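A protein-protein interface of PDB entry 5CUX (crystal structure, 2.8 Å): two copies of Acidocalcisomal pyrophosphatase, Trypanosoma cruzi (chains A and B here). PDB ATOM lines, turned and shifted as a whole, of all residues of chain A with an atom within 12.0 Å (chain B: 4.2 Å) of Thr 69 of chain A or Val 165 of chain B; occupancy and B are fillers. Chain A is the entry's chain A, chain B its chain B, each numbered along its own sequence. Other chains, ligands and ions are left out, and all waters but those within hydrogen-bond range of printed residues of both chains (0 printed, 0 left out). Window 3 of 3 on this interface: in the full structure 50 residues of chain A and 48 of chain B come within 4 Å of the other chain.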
ATOM      1  N   VAL A  63      -6.836  -2.298 -12.890  1.00  0.00           N
ATOM      2  CA  VAL A  63      -7.637  -2.857 -11.811  1.00  0.00           C
ATOM      3  C   VAL A  63      -8.660  -1.817 -11.478  1.00  0.00           C
ATOM      4  O   VAL A  63      -8.309  -0.671 -11.242  1.00  0.00           O
ATOM      5  CB  VAL A  63      -6.852  -3.134 -10.572  1.00  0.00           C
ATOM      6  CG1 VAL A  63      -7.726  -3.831  -9.604  1.00  0.00           C
ATOM      7  CG2 VAL A  63      -5.676  -3.961 -10.891  1.00  0.00           C
ATOM      8  N   ARG A  64      -9.927  -2.195 -11.479  1.00  0.00           N
ATOM      9  CA  ARG A  64     -10.970  -1.221 -11.200  1.00  0.00           C
ATOM     10  C   ARG A  64     -12.151  -1.806 -10.469  1.00  0.00           C
ATOM     11  O   ARG A  64     -12.568  -2.929 -10.762  1.00  0.00           O
ATOM     12  CB  ARG A  64     -11.548  -0.638 -12.474  1.00  0.00           C
ATOM     13  CG  ARG A  64     -10.625  -0.183 -13.490  1.00  0.00           C
ATOM     14  CD  ARG A  64     -11.489   0.610 -14.440  1.00  0.00           C
ATOM     15  NE  ARG A  64     -10.721   1.346 -15.441  1.00  0.00           N
ATOM     16  CZ  ARG A  64     -10.532   0.906 -16.685  1.00  0.00           C
ATOM     17  NH1 ARG A  64     -11.076  -0.270 -17.053  1.00  0.00           N
ATOM     18  NH2 ARG A  64      -9.799   1.633 -17.549  1.00  0.00           N
ATOM     19  N   ASP A  65     -12.714  -1.039  -9.547  1.00  0.00           N
ATOM     20  CA  ASP A  65     -13.901  -1.527  -8.880  1.00  0.00           C
ATOM     21  C   ASP A  65     -15.102  -0.746  -9.408  1.00  0.00           C
ATOM     22  O   ASP A  65     -14.978   0.111 -10.274  1.00  0.00           O
ATOM     23  CB  ASP A  65     -13.777  -1.436  -7.367  1.00  0.00           C
ATOM     24  CG  ASP A  65     -13.471  -0.067  -6.918  1.00  0.00           C
ATOM     25  OD1 ASP A  65     -13.614   0.858  -7.766  1.00  0.00           O
ATOM     26  OD2 ASP A  65     -13.095   0.066  -5.734  1.00  0.00           O
ATOM     27  N   LEU A  66     -16.266  -1.037  -8.884  1.00  0.00           N
ATOM     28  CA  LEU A  66     -17.448  -0.412  -9.414  1.00  0.00           C
ATOM     29  C   LEU A  66     -17.620   1.103  -9.210  1.00  0.00           C
ATOM     30  O   LEU A  66     -18.025   1.807 -10.134  1.00  0.00           O
ATOM     31  CB  LEU A  66     -18.632  -1.236  -8.916  1.00  0.00           C
ATOM     32  CG  LEU A  66     -18.311  -2.777  -8.932  1.00  0.00           C
ATOM     33  CD1 LEU A  66     -19.618  -3.562  -8.711  1.00  0.00           C
ATOM     34  CD2 LEU A  66     -17.675  -3.255 -10.266  1.00  0.00           C
ATOM     35  N   VAL A  67     -17.277   1.613  -8.032  1.00  0.00           N
ATOM     36  CA  VAL A  67     -17.389   3.041  -7.746  1.00  0.00           C
ATOM     37  C   VAL A  67     -16.063   3.416  -7.150  1.00  0.00           C
ATOM     38  O   VAL A  67     -15.730   2.897  -6.118  1.00  0.00           O
ATOM     39  CB  VAL A  67     -18.422   3.310  -6.652  1.00  0.00           C
ATOM     40  CG1 VAL A  67     -18.249   4.728  -6.116  1.00  0.00           C
ATOM     41  CG2 VAL A  67     -19.826   3.076  -7.171  1.00  0.00           C
ATOM     42  N   ARG A  68     -15.298   4.302  -7.762  1.00  0.00           N
ATOM     43  CA  ARG A  68     -13.997   4.703  -7.205  1.00  0.00           C
ATOM     44  C   ARG A  68     -14.205   5.758  -6.088  1.00  0.00           C
ATOM     45  O   ARG A  68     -14.835   6.801  -6.299  1.00  0.00           O
ATOM     46  CB  ARG A  68     -13.127   5.274  -8.344  1.00  0.00           C
ATOM     47  CG  ARG A  68     -11.721   5.706  -7.992  1.00  0.00           C
ATOM     48  CD  ARG A  68     -11.025   6.149  -9.246  1.00  0.00           C
ATOM     49  NE  ARG A  68      -9.595   6.302  -9.072  1.00  0.00           N
ATOM     50  CZ  ARG A  68      -9.003   7.423  -8.679  1.00  0.00           C
ATOM     51  NH1 ARG A  68      -9.734   8.513  -8.440  1.00  0.00           N
ATOM     52  NH2 ARG A  68      -7.682   7.442  -8.461  1.00  0.00           N
ATOM     53  N   THR A  69     -13.674   5.519  -4.898  1.00  0.00           N
ATOM     54  CA  THR A  69     -13.892   6.495  -3.876  1.00  0.00           C
ATOM     55  C   THR A  69     -12.673   7.352  -3.595  1.00  0.00           C
ATOM     56  O   THR A  69     -12.721   8.264  -2.743  1.00  0.00           O
ATOM     57  CB  THR A  69     -14.368   5.850  -2.606  1.00  0.00           C
ATOM     58  OG1 THR A  69     -13.346   5.006  -2.120  1.00  0.00           O
ATOM     59  CG2 THR A  69     -15.590   5.030  -2.865  1.00  0.00           C
ATOM     60  N   LYS A  70     -11.587   7.085  -4.309  1.00  0.00           N
ATOM     61  CA  LYS A  70     -10.359   7.872  -4.164  1.00  0.00           C
ATOM     62  C   LYS A  70     -10.593   9.242  -4.801  1.00  0.00           C
ATOM     63  O   LYS A  70     -11.448   9.385  -5.675  1.00  0.00           O
ATOM     64  CB  LYS A  70      -9.212   7.206  -4.902  1.00  0.00           C
ATOM     65  CG  LYS A  70      -8.829   5.860  -4.382  1.00  0.00           C
ATOM     66  CD  LYS A  70      -7.455   5.484  -4.881  1.00  0.00           C
ATOM     67  CE  LYS A  70      -6.839   4.437  -4.013  1.00  0.00           C
ATOM     68  NZ  LYS A  70      -7.493   3.139  -4.287  1.00  0.00           N
ATOM     69  N   PRO A  71      -9.813  10.261  -4.407  1.00  0.00           N
ATOM     70  CA  PRO A  71     -10.018  11.590  -5.007  1.00  0.00           C
ATOM     71  C   PRO A  71      -9.954  11.535  -6.525  1.00  0.00           C
ATOM     72  O   PRO A  71      -9.141  10.829  -7.127  1.00  0.00           O
ATOM     73  CB  PRO A  71      -8.883  12.411  -4.435  1.00  0.00           C
ATOM     74  CG  PRO A  71      -8.522  11.693  -3.170  1.00  0.00           C
ATOM     75  CD  PRO A  71      -8.643  10.254  -3.510  1.00  0.00           C
ATOM     76  N   ALA A  72     -10.831  12.280  -7.159  1.00  0.00           N
ATOM     77  CA  ALA A  72     -10.840  12.273  -8.593  1.00  0.00           C
ATOM     78  C   ALA A  72      -9.559  12.947  -9.014  1.00  0.00           C
ATOM     79  O   ALA A  72      -9.138  12.780 -10.133  1.00  0.00           O
ATOM     80  CB  ALA A  72     -12.051  13.022  -9.125  1.00  0.00           C
ATOM     81  N   SER A  73      -8.915  13.688  -8.118  1.00  0.00           N
ATOM     82  CA  SER A  73      -7.679  14.380  -8.487  1.00  0.00           C
ATOM     83  C   SER A  73      -6.459  13.451  -8.466  1.00  0.00           C
ATOM     84  O   SER A  73      -5.441  13.760  -9.056  1.00  0.00           O
ATOM     85  CB  SER A  73      -7.416  15.521  -7.533  1.00  0.00           C
ATOM     86  OG  SER A  73      -6.954  14.986  -6.298  1.00  0.00           O
ATOM     87  N   LEU A  74      -6.534  12.337  -7.744  1.00  0.00           N
ATOM     88  CA  LEU A  74      -5.438  11.366  -7.713  1.00  0.00           C
ATOM     89  C   LEU A  74      -5.421  10.494  -8.982  1.00  0.00           C
ATOM     90  O   LEU A  74      -6.318   9.716  -9.245  1.00  0.00           O
ATOM     91  CB  LEU A  74      -5.603  10.464  -6.509  1.00  0.00           C
ATOM     92  CG  LEU A  74      -4.710   9.229  -6.498  1.00  0.00           C
ATOM     93  CD1 LEU A  74      -3.274   9.615  -6.565  1.00  0.00           C
ATOM     94  CD2 LEU A  74      -4.987   8.456  -5.240  1.00  0.00           C
ATOM     95  N   PRO A  75      -4.367  10.580  -9.768  1.00  0.00           N
ATOM     96  CA  PRO A  75      -4.334   9.768 -10.993  1.00  0.00           C
ATOM     97  C   PRO A  75      -4.328   8.293 -10.709  1.00  0.00           C
ATOM     98  O   PRO A  75      -3.769   7.865  -9.721  1.00  0.00           O
ATOM     99  CB  PRO A  75      -3.040  10.193 -11.653  1.00  0.00           C
ATOM    100  CG  PRO A  75      -2.609  11.458 -10.890  1.00  0.00           C
ATOM    101  CD  PRO A  75      -3.064  11.205  -9.504  1.00  0.00           C
ATOM    102  N   MET A  76      -4.926   7.511 -11.596  1.00  0.00           N
ATOM    103  CA  MET A  76      -4.985   6.063 -11.416  1.00  0.00           C
ATOM    104  C   MET A  76      -3.707   5.351 -11.799  1.00  0.00           C
ATOM    105  O   MET A  76      -3.095   5.659 -12.819  1.00  0.00           O
ATOM    106  CB  MET A  76      -6.105   5.483 -12.228  1.00  0.00           C
ATOM    107  CG  MET A  76      -7.467   5.916 -11.758  1.00  0.00           C
ATOM    108  SD  MET A  76      -8.751   5.685 -13.023  1.00  0.00           S
ATOM    109  CE  MET A  76      -8.629   7.466 -13.863  1.00  0.00           C
ATOM    110  N   ARG A  78      -3.060   1.336 -10.933  1.00  0.00           N
ATOM    111  CA  ARG A  78      -3.158  -0.008 -10.332  1.00  0.00           C
ATOM    112  C   ARG A  78      -3.352  -0.911 -11.525  1.00  0.00           C
ATOM    113  O   ARG A  78      -4.419  -0.946 -12.108  1.00  0.00           O
ATOM    114  CB  ARG A  78      -4.357  -0.168  -9.348  1.00  0.00           C
ATOM    115  CG  ARG A  78      -3.964  -0.202  -7.823  1.00  0.00           C
ATOM    116  CD  ARG A  78      -5.118  -0.143  -6.670  1.00  0.00           C
ATOM    117  NE  ARG A  78      -4.507  -0.137  -5.299  1.00  0.00           N
ATOM    118  CZ  ARG A  78      -5.117  -0.073  -4.091  1.00  0.00           C
ATOM    119  NH1 ARG A  78      -4.377  -0.084  -2.971  1.00  0.00           N
ATOM    120  NH2 ARG A  78      -6.443   0.010  -3.962  1.00  0.00           N
ATOM    121  N   LEU B  23     -16.748   8.797  -7.514  1.00  0.00           N
ATOM    122  CA  LEU B  23     -17.495   9.486  -6.487  1.00  0.00           C
ATOM    123  C   LEU B  23     -16.937  10.890  -6.427  1.00  0.00           C
ATOM    124  O   LEU B  23     -15.730  11.058  -6.496  1.00  0.00           O
ATOM    125  CB  LEU B  23     -17.341   8.775  -5.121  1.00  0.00           C
ATOM    126  CG  LEU B  23     -18.329   9.225  -4.000  1.00  0.00           C
ATOM    127  CD1 LEU B  23     -19.806   8.943  -4.390  1.00  0.00           C
ATOM    128  CD2 LEU B  23     -17.983   8.519  -2.707  1.00  0.00           C
ATOM    129  N   ILE B  59     -23.731   4.149  -2.549  1.00  0.00           N
ATOM    130  CA  ILE B  59     -22.335   3.822  -2.457  1.00  0.00           C
ATOM    131  C   ILE B  59     -22.336   2.424  -1.946  1.00  0.00           C
ATOM    132  O   ILE B  59     -22.855   2.160  -0.886  1.00  0.00           O
ATOM    133  CB  ILE B  59     -21.640   4.756  -1.437  1.00  0.00           C
ATOM    134  CG1 ILE B  59     -21.602   6.171  -2.001  1.00  0.00           C
ATOM    135  CG2 ILE B  59     -20.240   4.229  -1.039  1.00  0.00           C
ATOM    136  CD1 ILE B  59     -20.891   7.092  -1.090  1.00  0.00           C
ATOM    137  N   ASN B  80     -16.991  -0.012   2.494  1.00  0.00           N
ATOM    138  CA  ASN B  80     -16.802   1.406   2.335  1.00  0.00           C
ATOM    139  C   ASN B  80     -17.195   2.022   3.667  1.00  0.00           C
ATOM    140  O   ASN B  80     -18.002   1.482   4.410  1.00  0.00           O
ATOM    141  CB  ASN B  80     -17.669   1.975   1.229  1.00  0.00           C
ATOM    142  CG  ASN B  80     -16.985   1.958  -0.085  1.00  0.00           C
ATOM    143  OD1 ASN B  80     -15.827   2.303  -0.168  1.00  0.00           O
ATOM    144  ND2 ASN B  80     -17.695   1.576  -1.135  1.00  0.00           N
ATOM    145  N   PHE B  81     -16.609   3.170   3.945  1.00  0.00           N
ATOM    146  CA  PHE B  81     -16.835   3.906   5.164  1.00  0.00           C
ATOM    147  C   PHE B  81     -16.985   5.395   4.810  1.00  0.00           C
ATOM    148  O   PHE B  81     -16.146   5.969   4.084  1.00  0.00           O
ATOM    149  CB  PHE B  81     -15.636   3.684   6.067  1.00  0.00           C
ATOM    150  CG  PHE B  81     -15.507   4.675   7.174  1.00  0.00           C
ATOM    151  CD1 PHE B  81     -16.242   4.541   8.335  1.00  0.00           C
ATOM    152  CD2 PHE B  81     -14.570   5.691   7.096  1.00  0.00           C
ATOM    153  CE1 PHE B  81     -16.045   5.394   9.415  1.00  0.00           C
ATOM    154  CE2 PHE B  81     -14.373   6.532   8.159  1.00  0.00           C
ATOM    155  CZ  PHE B  81     -15.123   6.374   9.329  1.00  0.00           C
ATOM    156  N   ILE B  82     -18.058   6.002   5.315  1.00  0.00           N
ATOM    157  CA  ILE B  82     -18.366   7.420   5.106  1.00  0.00           C
ATOM    158  C   ILE B  82     -18.040   8.188   6.377  1.00  0.00           C
ATOM    159  O   ILE B  82     -18.761   8.059   7.356  1.00  0.00           O
ATOM    160  CB  ILE B  82     -19.857   7.623   4.803  1.00  0.00           C
ATOM    161  CG1 ILE B  82     -20.276   6.640   3.707  1.00  0.00           C
ATOM    162  CG2 ILE B  82     -20.120   9.025   4.347  1.00  0.00           C
ATOM    163  CD1 ILE B  82     -21.743   6.612   3.452  1.00  0.00           C
ATOM    164  N   GLY B 163     -17.095  13.811   5.197  1.00  0.00           N
ATOM    165  CA  GLY B 163     -17.804  13.158   4.109  1.00  0.00           C
ATOM    166  C   GLY B 163     -16.928  12.317   3.210  1.00  0.00           C
ATOM    167  O   GLY B 163     -17.411  11.761   2.225  1.00  0.00           O
ATOM    168  N   GLN B 164     -15.640  12.218   3.545  1.00  0.00           N
ATOM    169  CA  GLN B 164     -14.685  11.431   2.758  1.00  0.00           C
ATOM    170  C   GLN B 164     -15.002   9.941   2.868  1.00  0.00           C
ATOM    171  O   GLN B 164     -15.303   9.448   3.941  1.00  0.00           O
ATOM    172  CB  GLN B 164     -13.271  11.691   3.251  1.00  0.00           C
ATOM    173  CG  GLN B 164     -12.206  11.033   2.389  1.00  0.00           C
ATOM    174  CD  GLN B 164     -10.819  11.239   2.920  1.00  0.00           C
ATOM    175  OE1 GLN B 164     -10.399  12.355   3.169  1.00  0.00           O
ATOM    176  NE2 GLN B 164     -10.101  10.165   3.109  1.00  0.00           N
ATOM    177  N   VAL B 165     -14.923   9.215   1.762  1.00  0.00           N
ATOM    178  CA  VAL B 165     -15.259   7.783   1.772  1.00  0.00           C
ATOM    179  C   VAL B 165     -14.051   6.939   1.388  1.00  0.00           C
ATOM    180  O   VAL B 165     -13.306   7.297   0.480  1.00  0.00           O
ATOM    181  CB  VAL B 165     -16.451   7.509   0.764  1.00  0.00           C
ATOM    182  CG1 VAL B 165     -16.645   6.020   0.512  1.00  0.00           C
ATOM    183  CG2 VAL B 165     -17.717   8.177   1.290  1.00  0.00           C
ATOM    184  N   GLY B 166     -13.871   5.819   2.080  1.00  0.00           N
ATOM    185  CA  GLY B 166     -12.761   4.929   1.791  1.00  0.00           C
ATOM    186  C   GLY B 166     -12.954   3.492   2.277  1.00  0.00           C
ATOM    187  O   GLY B 166     -13.745   3.207   3.181  1.00  0.00           O
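The backbone carbonyl oxygen (O) of Val 165 of chain B lies within hydrogen-bond range of the side-chain hydroxyl (OG1) of Thr 69 of chain A (3.5 Å).
The backbone NH (N) of Leu 23 of chain B lies within hydrogen-bond range of the backbone carbonyl oxygen (O) of Arg 68 of chain A (3.0 Å).
O of Pro 71 of chain A is in hydrogen-bond range of NH1 of Arg 68 of chain A (2.7 Å).
The guanidinium group (NH2) of Arg 68 of chain A sits at hydrogen-bond distance from the backbone carbonyl oxygen (O) of Leu 74 of chain A, 2.8 Å away.
The backbone carbonyl oxygen (O) of Lys 70 of chain A is in hydrogen-bond range of the guanidinium group (NH1) of Arg 68 of chain A (3.4 Å).
The backbone NH (N) of Phe 81 of chain B sits at hydrogen-bond distance from the backbone carbonyl oxygen (O) of Gly 166 of chain B, 3.0 Å away.
Among the printed residues, pairs that only touch across the chains: Thr 69 of chain A with Asn 80 of chain B (3.8 Å) and Thr 69 of chain A with Gly 166 of chain B (3.96 Å).
Printed residues of chain B within 4 Å of Arg 68 of chain A: Leu 23.
Of chain B, only Asn 80 (3.8 Å), Val 165 (3.4 Å) and Gly 166 (3.96 Å) come within 4 Å of Thr 69 of chain A.
Arg 78 of chain A touches none of the printed residues of chain B.
Of chain A, only Arg 68 (3.0 Å) comes within 4 Å of Leu 23 of chain B.
Asn 80 of chain B touches one residue of chain A.
No residue of chain A comes within 4 Å of Ile 82 of chain B.
No residue of chain A comes within 4 Å of Gly 163 of chain B.
No residue of chain A comes within 4 Å of Gln 164 of chain B.
Val 165 of chain B touches one residue of chain A.
The nearest printed residue of chain B that does not touch Thr 69 of chain A is Leu 23 of chain B (4.2 Å).
Of the 9 printed residues of chain B, 4 touch a printed residue of chain A.
Along chain B the printed residues that touch a printed residue of chain A span positions 23 to 166.
Of the 15 printed residues of chain A, 2 touch a printed residue of chain B.
No position is printed for both chains.
Of the 4 pairs that touch across the chains among the printed residues, none has its exchanged pair printed and touching as well.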
